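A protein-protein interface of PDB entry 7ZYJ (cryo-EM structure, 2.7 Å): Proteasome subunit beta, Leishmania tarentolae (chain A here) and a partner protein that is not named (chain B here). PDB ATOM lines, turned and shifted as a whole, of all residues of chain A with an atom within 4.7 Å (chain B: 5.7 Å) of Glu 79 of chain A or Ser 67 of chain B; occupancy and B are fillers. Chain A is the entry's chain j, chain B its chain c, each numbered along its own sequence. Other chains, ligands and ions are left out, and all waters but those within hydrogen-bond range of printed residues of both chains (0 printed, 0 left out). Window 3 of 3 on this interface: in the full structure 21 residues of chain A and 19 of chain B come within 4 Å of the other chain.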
ATOM      1  N   LYS A  75     -14.724  20.532 -26.170  1.00  0.00           N
ATOM      2  CA  LYS A  75     -14.329  21.708 -25.404  1.00  0.00           C
ATOM      3  C   LYS A  75     -14.168  22.932 -26.296  1.00  0.00           C
ATOM      4  O   LYS A  75     -14.341  24.063 -25.828  1.00  0.00           O
ATOM      5  CB  LYS A  75     -13.037  21.431 -24.638  1.00  0.00           C
ATOM      6  CG  LYS A  75     -12.785  22.398 -23.497  1.00  0.00           C
ATOM      7  CD  LYS A  75     -11.609  21.959 -22.646  1.00  0.00           C
ATOM      8  CE  LYS A  75     -11.121  23.092 -21.761  1.00  0.00           C
ATOM      9  NZ  LYS A  75     -12.227  23.697 -20.969  1.00  0.00           N
ATOM     10  N   LEU A  76     -13.832  22.733 -27.571  1.00  0.00           N
ATOM     11  CA  LEU A  76     -13.765  23.862 -28.494  1.00  0.00           C
ATOM     12  C   LEU A  76     -15.159  24.357 -28.855  1.00  0.00           C
ATOM     13  O   LEU A  76     -15.454  25.552 -28.739  1.00  0.00           O
ATOM     14  CB  LEU A  76     -12.988  23.467 -29.748  1.00  0.00           C
ATOM     15  CG  LEU A  76     -11.465  23.524 -29.640  1.00  0.00           C
ATOM     16  CD1 LEU A  76     -10.824  23.001 -30.911  1.00  0.00           C
ATOM     17  CD2 LEU A  76     -11.003  24.940 -29.343  1.00  0.00           C
ATOM     18  N   ARG A  77     -16.031  23.450 -29.300  1.00  0.00           N
ATOM     19  CA  ARG A  77     -17.402  23.824 -29.629  1.00  0.00           C
ATOM     20  C   ARG A  77     -18.146  24.314 -28.395  1.00  0.00           C
ATOM     21  O   ARG A  77     -18.586  25.467 -28.330  1.00  0.00           O
ATOM     22  CB  ARG A  77     -18.129  22.639 -30.264  1.00  0.00           C
ATOM     23  CG  ARG A  77     -17.750  22.380 -31.707  1.00  0.00           C
ATOM     24  CD  ARG A  77     -18.905  21.762 -32.474  1.00  0.00           C
ATOM     25  NE  ARG A  77     -18.444  20.776 -33.444  1.00  0.00           N
ATOM     26  CZ  ARG A  77     -18.140  19.520 -33.149  1.00  0.00           C
ATOM     27  NH1 ARG A  77     -18.235  19.056 -31.914  1.00  0.00           N
ATOM     28  NH2 ARG A  77     -17.727  18.709 -34.118  1.00  0.00           N
ATOM     29  N   GLU A  78     -18.298  23.444 -27.400  1.00  0.00           N
ATOM     30  CA  GLU A  78     -18.938  23.818 -26.145  1.00  0.00           C
ATOM     31  C   GLU A  78     -17.881  24.408 -25.223  1.00  0.00           C
ATOM     32  O   GLU A  78     -16.943  23.717 -24.817  1.00  0.00           O
ATOM     33  CB  GLU A  78     -19.608  22.610 -25.500  1.00  0.00           C
ATOM     34  CG  GLU A  78     -20.421  21.772 -26.460  1.00  0.00           C
ATOM     35  CD  GLU A  78     -21.440  20.912 -25.751  1.00  0.00           C
ATOM     36  OE1 GLU A  78     -21.588  21.056 -24.520  1.00  0.00           O
ATOM     37  OE2 GLU A  78     -22.090  20.089 -26.424  1.00  0.00           O
ATOM     38  N   GLU A  79     -18.035  25.684 -24.885  1.00  0.00           N
ATOM     39  CA  GLU A  79     -17.069  26.354 -24.027  1.00  0.00           C
ATOM     40  C   GLU A  79     -17.227  25.876 -22.590  1.00  0.00           C
ATOM     41  O   GLU A  79     -17.707  26.623 -21.734  1.00  0.00           O
ATOM     42  CB  GLU A  79     -17.246  27.868 -24.117  1.00  0.00           C
ATOM     43  CG  GLU A  79     -17.111  28.411 -25.527  1.00  0.00           C
ATOM     44  CD  GLU A  79     -16.584  29.827 -25.562  1.00  0.00           C
ATOM     45  OE1 GLU A  79     -16.708  30.478 -26.618  1.00  0.00           O
ATOM     46  OE2 GLU A  79     -16.044  30.289 -24.534  1.00  0.00           O
ATOM     47  N   ARG A  80     -16.846  24.629 -22.324  1.00  0.00           N
ATOM     48  CA  ARG A  80     -16.956  24.039 -20.996  1.00  0.00           C
ATOM     49  C   ARG A  80     -16.307  22.665 -21.027  1.00  0.00           C
ATOM     50  O   ARG A  80     -16.147  22.060 -22.090  1.00  0.00           O
ATOM     51  CB  ARG A  80     -18.414  23.925 -20.537  1.00  0.00           C
ATOM     52  CG  ARG A  80     -19.296  23.120 -21.473  1.00  0.00           C
ATOM     53  CD  ARG A  80     -20.579  22.692 -20.789  1.00  0.00           C
ATOM     54  NE  ARG A  80     -21.452  21.952 -21.690  1.00  0.00           N
ATOM     55  CZ  ARG A  80     -22.497  21.236 -21.300  1.00  0.00           C
ATOM     56  NH1 ARG A  80     -22.831  21.140 -20.024  1.00  0.00           N
ATOM     57  NH2 ARG A  80     -23.225  20.599 -22.213  1.00  0.00           N
ATOM     58  N   MET B  61     -21.170  31.712 -20.885  1.00  0.00           N
ATOM     59  CA  MET B  61     -20.317  30.563 -21.137  1.00  0.00           C
ATOM     60  C   MET B  61     -19.304  30.388 -20.016  1.00  0.00           C
ATOM     61  O   MET B  61     -18.669  31.352 -19.581  1.00  0.00           O
ATOM     62  CB  MET B  61     -19.586  30.723 -22.469  1.00  0.00           C
ATOM     63  CG  MET B  61     -20.484  30.904 -23.672  1.00  0.00           C
ATOM     64  SD  MET B  61     -21.139  29.336 -24.268  1.00  0.00           S
ATOM     65  CE  MET B  61     -21.234  29.672 -26.022  1.00  0.00           C
ATOM     66  N   GLN B  62     -19.159  29.151 -19.551  1.00  0.00           N
ATOM     67  CA  GLN B  62     -17.980  28.773 -18.796  1.00  0.00           C
ATOM     68  C   GLN B  62     -16.764  28.851 -19.723  1.00  0.00           C
ATOM     69  O   GLN B  62     -16.894  28.959 -20.945  1.00  0.00           O
ATOM     70  CB  GLN B  62     -18.168  27.368 -18.217  1.00  0.00           C
ATOM     71  CG  GLN B  62     -17.068  26.871 -17.295  1.00  0.00           C
ATOM     72  CD  GLN B  62     -17.369  25.499 -16.726  1.00  0.00           C
ATOM     73  OE1 GLN B  62     -18.449  24.948 -16.942  1.00  0.00           O
ATOM     74  NE2 GLN B  62     -16.412  24.938 -15.998  1.00  0.00           N
ATOM     75  N   ASP B  63     -15.567  28.837 -19.134  1.00  0.00           N
ATOM     76  CA  ASP B  63     -14.323  28.787 -19.903  1.00  0.00           C
ATOM     77  C   ASP B  63     -14.250  29.968 -20.879  1.00  0.00           C
ATOM     78  O   ASP B  63     -14.262  29.816 -22.101  1.00  0.00           O
ATOM     79  CB  ASP B  63     -14.202  27.442 -20.634  1.00  0.00           C
ATOM     80  CG  ASP B  63     -12.844  27.238 -21.284  1.00  0.00           C
ATOM     81  OD1 ASP B  63     -11.988  28.144 -21.207  1.00  0.00           O
ATOM     82  OD2 ASP B  63     -12.636  26.160 -21.879  1.00  0.00           O
ATOM     83  N   LYS B  64     -14.186  31.163 -20.291  1.00  0.00           N
ATOM     84  CA  LYS B  64     -14.288  32.398 -21.059  1.00  0.00           C
ATOM     85  C   LYS B  64     -12.983  32.730 -21.771  1.00  0.00           C
ATOM     86  O   LYS B  64     -12.479  33.852 -21.663  1.00  0.00           O
ATOM     87  CB  LYS B  64     -14.690  33.554 -20.143  1.00  0.00           C
ATOM     88  CG  LYS B  64     -16.020  33.351 -19.439  1.00  0.00           C
ATOM     89  CD  LYS B  64     -16.347  34.521 -18.530  1.00  0.00           C
ATOM     90  CE  LYS B  64     -17.682  34.317 -17.836  1.00  0.00           C
ATOM     91  NZ  LYS B  64     -17.636  33.175 -16.881  1.00  0.00           N
ATOM     92  N   ASN B  65     -12.435  31.767 -22.503  1.00  0.00           N
ATOM     93  CA  ASN B  65     -11.227  32.014 -23.280  1.00  0.00           C
ATOM     94  C   ASN B  65     -11.248  31.362 -24.654  1.00  0.00           C
ATOM     95  O   ASN B  65     -10.222  31.392 -25.337  1.00  0.00           O
ATOM     96  CB  ASN B  65      -9.992  31.536 -22.497  1.00  0.00           C
ATOM     97  CG  ASN B  65      -9.369  32.636 -21.664  1.00  0.00           C
ATOM     98  OD1 ASN B  65      -9.384  33.805 -22.048  1.00  0.00           O
ATOM     99  ND2 ASN B  65      -8.814  32.268 -20.516  1.00  0.00           N
ATOM    100  N   THR B  66     -12.362  30.773 -25.086  1.00  0.00           N
ATOM    101  CA  THR B  66     -12.411  30.064 -26.358  1.00  0.00           C
ATOM    102  C   THR B  66     -12.847  30.969 -27.505  1.00  0.00           C
ATOM    103  O   THR B  66     -12.218  30.975 -28.567  1.00  0.00           O
ATOM    104  CB  THR B  66     -13.349  28.858 -26.251  1.00  0.00           C
ATOM    105  OG1 THR B  66     -12.891  27.983 -25.214  1.00  0.00           O
ATOM    106  CG2 THR B  66     -13.395  28.097 -27.566  1.00  0.00           C
ATOM    107  N   SER B  67     -13.913  31.739 -27.315  1.00  0.00           N
ATOM    108  CA  SER B  67     -14.407  32.604 -28.380  1.00  0.00           C
ATOM    109  C   SER B  67     -14.991  33.866 -27.769  1.00  0.00           C
ATOM    110  O   SER B  67     -15.727  33.796 -26.780  1.00  0.00           O
ATOM    111  CB  SER B  67     -15.454  31.885 -29.232  1.00  0.00           C
ATOM    112  OG  SER B  67     -16.672  31.729 -28.522  1.00  0.00           O
ATOM    113  N   GLY B  68     -14.660  35.009 -28.358  1.00  0.00           N
ATOM    114  CA  GLY B  68     -15.261  36.274 -28.013  1.00  0.00           C
ATOM    115  C   GLY B  68     -16.179  36.773 -29.108  1.00  0.00           C
ATOM    116  O   GLY B  68     -16.626  36.017 -29.980  1.00  0.00           O
ATOM    117  N   GLU B  69     -16.465  38.073 -29.067  1.00  0.00           N
ATOM    118  CA  GLU B  69     -17.282  38.677 -30.110  1.00  0.00           C
ATOM    119  C   GLU B  69     -16.519  38.851 -31.417  1.00  0.00           C
ATOM    120  O   GLU B  69     -17.146  38.995 -32.472  1.00  0.00           O
ATOM    121  CB  GLU B  69     -17.823  40.029 -29.638  1.00  0.00           C
ATOM    122  CG  GLU B  69     -18.981  40.561 -30.469  1.00  0.00           C
ATOM    123  CD  GLU B  69     -19.430  41.941 -30.032  1.00  0.00           C
ATOM    124  OE1 GLU B  69     -19.765  42.110 -28.842  1.00  0.00           O
ATOM    125  OE2 GLU B  69     -19.456  42.855 -30.884  1.00  0.00           O
ATOM    126  N   MET B  71     -12.891  37.393 -31.596  1.00  0.00           N
ATOM    127  CA  MET B  71     -11.697  36.563 -31.536  1.00  0.00           C
ATOM    128  C   MET B  71     -12.042  35.167 -31.038  1.00  0.00           C
ATOM    129  O   MET B  71     -12.795  35.009 -30.072  1.00  0.00           O
ATOM    130  CB  MET B  71     -10.653  37.211 -30.628  1.00  0.00           C
ATOM    131  CG  MET B  71     -10.289  38.603 -31.097  1.00  0.00           C
ATOM    132  SD  MET B  71      -9.636  39.678 -29.817  1.00  0.00           S
ATOM    133  CE  MET B  71      -8.912  40.950 -30.841  1.00  0.00           C
ATOM    134  N   TYR B  72     -11.482  34.156 -31.698  1.00  0.00           N
ATOM    135  CA  TYR B  72     -11.822  32.766 -31.441  1.00  0.00           C
ATOM    136  C   TYR B  72     -10.554  31.945 -31.253  1.00  0.00           C
ATOM    137  O   TYR B  72      -9.458  32.354 -31.642  1.00  0.00           O
ATOM    138  CB  TYR B  72     -12.662  32.178 -32.583  1.00  0.00           C
ATOM    139  CG  TYR B  72     -13.759  33.099 -33.064  1.00  0.00           C
ATOM    140  CD1 TYR B  72     -15.019  33.072 -32.481  1.00  0.00           C
ATOM    141  CD2 TYR B  72     -13.535  33.999 -34.097  1.00  0.00           C
ATOM    142  CE1 TYR B  72     -16.023  33.914 -32.915  1.00  0.00           C
ATOM    143  CE2 TYR B  72     -14.533  34.843 -34.536  1.00  0.00           C
ATOM    144  CZ  TYR B  72     -15.775  34.797 -33.943  1.00  0.00           C
ATOM    145  OH  TYR B  72     -16.772  35.637 -34.379  1.00  0.00           O
ATOM    146  N   LYS B  73     -10.716  30.781 -30.633  1.00  0.00           N
ATOM    147  CA  LYS B  73      -9.624  29.841 -30.427  1.00  0.00           C
ATOM    148  C   LYS B  73      -9.759  28.680 -31.402  1.00  0.00           C
ATOM    149  O   LYS B  73     -10.809  28.034 -31.463  1.00  0.00           O
ATOM    150  CB  LYS B  73      -9.614  29.323 -28.988  1.00  0.00           C
ATOM    151  CG  LYS B  73      -8.683  28.150 -28.760  1.00  0.00           C
ATOM    152  CD  LYS B  73      -8.882  27.539 -27.385  1.00  0.00           C
ATOM    153  CE  LYS B  73      -8.230  28.379 -26.304  1.00  0.00           C
ATOM    154  NZ  LYS B  73      -8.390  27.763 -24.960  1.00  0.00           N
ATOM    155  N   ARG B  97     -10.479  24.141 -36.835  1.00  0.00           N
ATOM    156  CA  ARG B  97     -10.406  23.326 -35.627  1.00  0.00           C
ATOM    157  C   ARG B  97     -10.360  21.843 -35.972  1.00  0.00           C
ATOM    158  O   ARG B  97      -9.583  21.081 -35.382  1.00  0.00           O
ATOM    159  CB  ARG B  97     -11.594  23.625 -34.717  1.00  0.00           C
ATOM    160  CG  ARG B  97     -11.619  25.037 -34.167  1.00  0.00           C
ATOM    161  CD  ARG B  97     -12.924  25.309 -33.447  1.00  0.00           C
ATOM    162  NE  ARG B  97     -12.861  26.520 -32.640  1.00  0.00           N
ATOM    163  CZ  ARG B  97     -13.908  27.082 -32.054  1.00  0.00           C
ATOM    164  NH1 ARG B  97     -15.121  26.566 -32.166  1.00  0.00           N
ATOM    165  NH2 ARG B  97     -13.735  28.189 -31.338  1.00  0.00           N
ATOM    166  N   ILE B 248      -8.324  35.671 -23.735  1.00  0.00           N
ATOM    167  CA  ILE B 248      -9.089  36.849 -24.122  1.00  0.00           C
ATOM    168  C   ILE B 248      -9.249  37.745 -22.903  1.00  0.00           C
ATOM    169  O   ILE B 248      -9.712  37.298 -21.846  1.00  0.00           O
ATOM    170  CB  ILE B 248     -10.458  36.460 -24.710  1.00  0.00           C
ATOM    171  CG1 ILE B 248     -10.278  35.507 -25.893  1.00  0.00           C
ATOM    172  CG2 ILE B 248     -11.227  37.697 -25.137  1.00  0.00           C
ATOM    173  CD1 ILE B 248     -11.573  34.922 -26.403  1.00  0.00           C
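Of the printed residues of chain B, Leu 76 of chain A touches Thr 66, Lys 73 and Arg 97.
Glu 79 of chain A touches four residues of chain B.
Printed residues of chain A within 4 Å of Thr 66 of chain B: Leu 76 and Glu 79.
Of the printed residues of chain A, Ser 67 of chain B touches Glu 79 (2.3 Å).
The nearest printed residue of chain A that does not touch Ser 67 of chain B is Leu 76 of chain A (6.3 Å).
Of the 6 printed residues of chain A, 4 touch a printed residue of chain B.
Printed residues of chain A that touch a printed residue of chain B: Lys 75, Leu 76, Glu 79 and Arg 80.
Hydrophobic or aromatic side chains of chain A within 4 Å of the printed part of chain B: Leu 76.
Thr 66 of chain B touches Leu 76 of chain A (CG2 to O, 3.5 Å).
CD2 of Leu 76 of chain A touches O of Lys 73 of chain B, 3.8 Å away.
Arg 97 of chain B touches Leu 76 of chain A (NH1 to O, 3.6 Å).
Glu 79 of chain A touches Thr 66 of chain B.
CB of Arg 80 of chain A touches OE1 of Gln 62 of chain B, 3.7 Å away.
OE1 of Glu 79 of chain A lies within hydrogen-bond range of N of Ser 67 of chain B, 3.1 Å away.
The backbone carbonyl oxygen (O) of Gln 62 of chain B lies close to the backbone carbonyl oxygen (O) of Glu 79 of chain A (2.6 Å).
NZ of Lys 75 of chain A lies within salt-bridge range of OD2 of Asp 63 of chain B, 2.7 Å away.
OE2 of Glu 79 of chain A lies close to O of Asp 63 of chain B (3.1 Å).
The backbone carbonyl oxygen of Lys 73 of chain B sits at hydrogen-bond distance from the guanidinium group of Arg 97 of chain B (2.8 Å).
The guanidinium group (NH2) of Arg 80 of chain A lies within salt-bridge range of the side-chain carboxylate (OE1) of Glu 78 of chain A (2.9 Å).
O of Thr 66 of chain B lies within hydrogen-bond range of N of Lys 73 of chain B.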
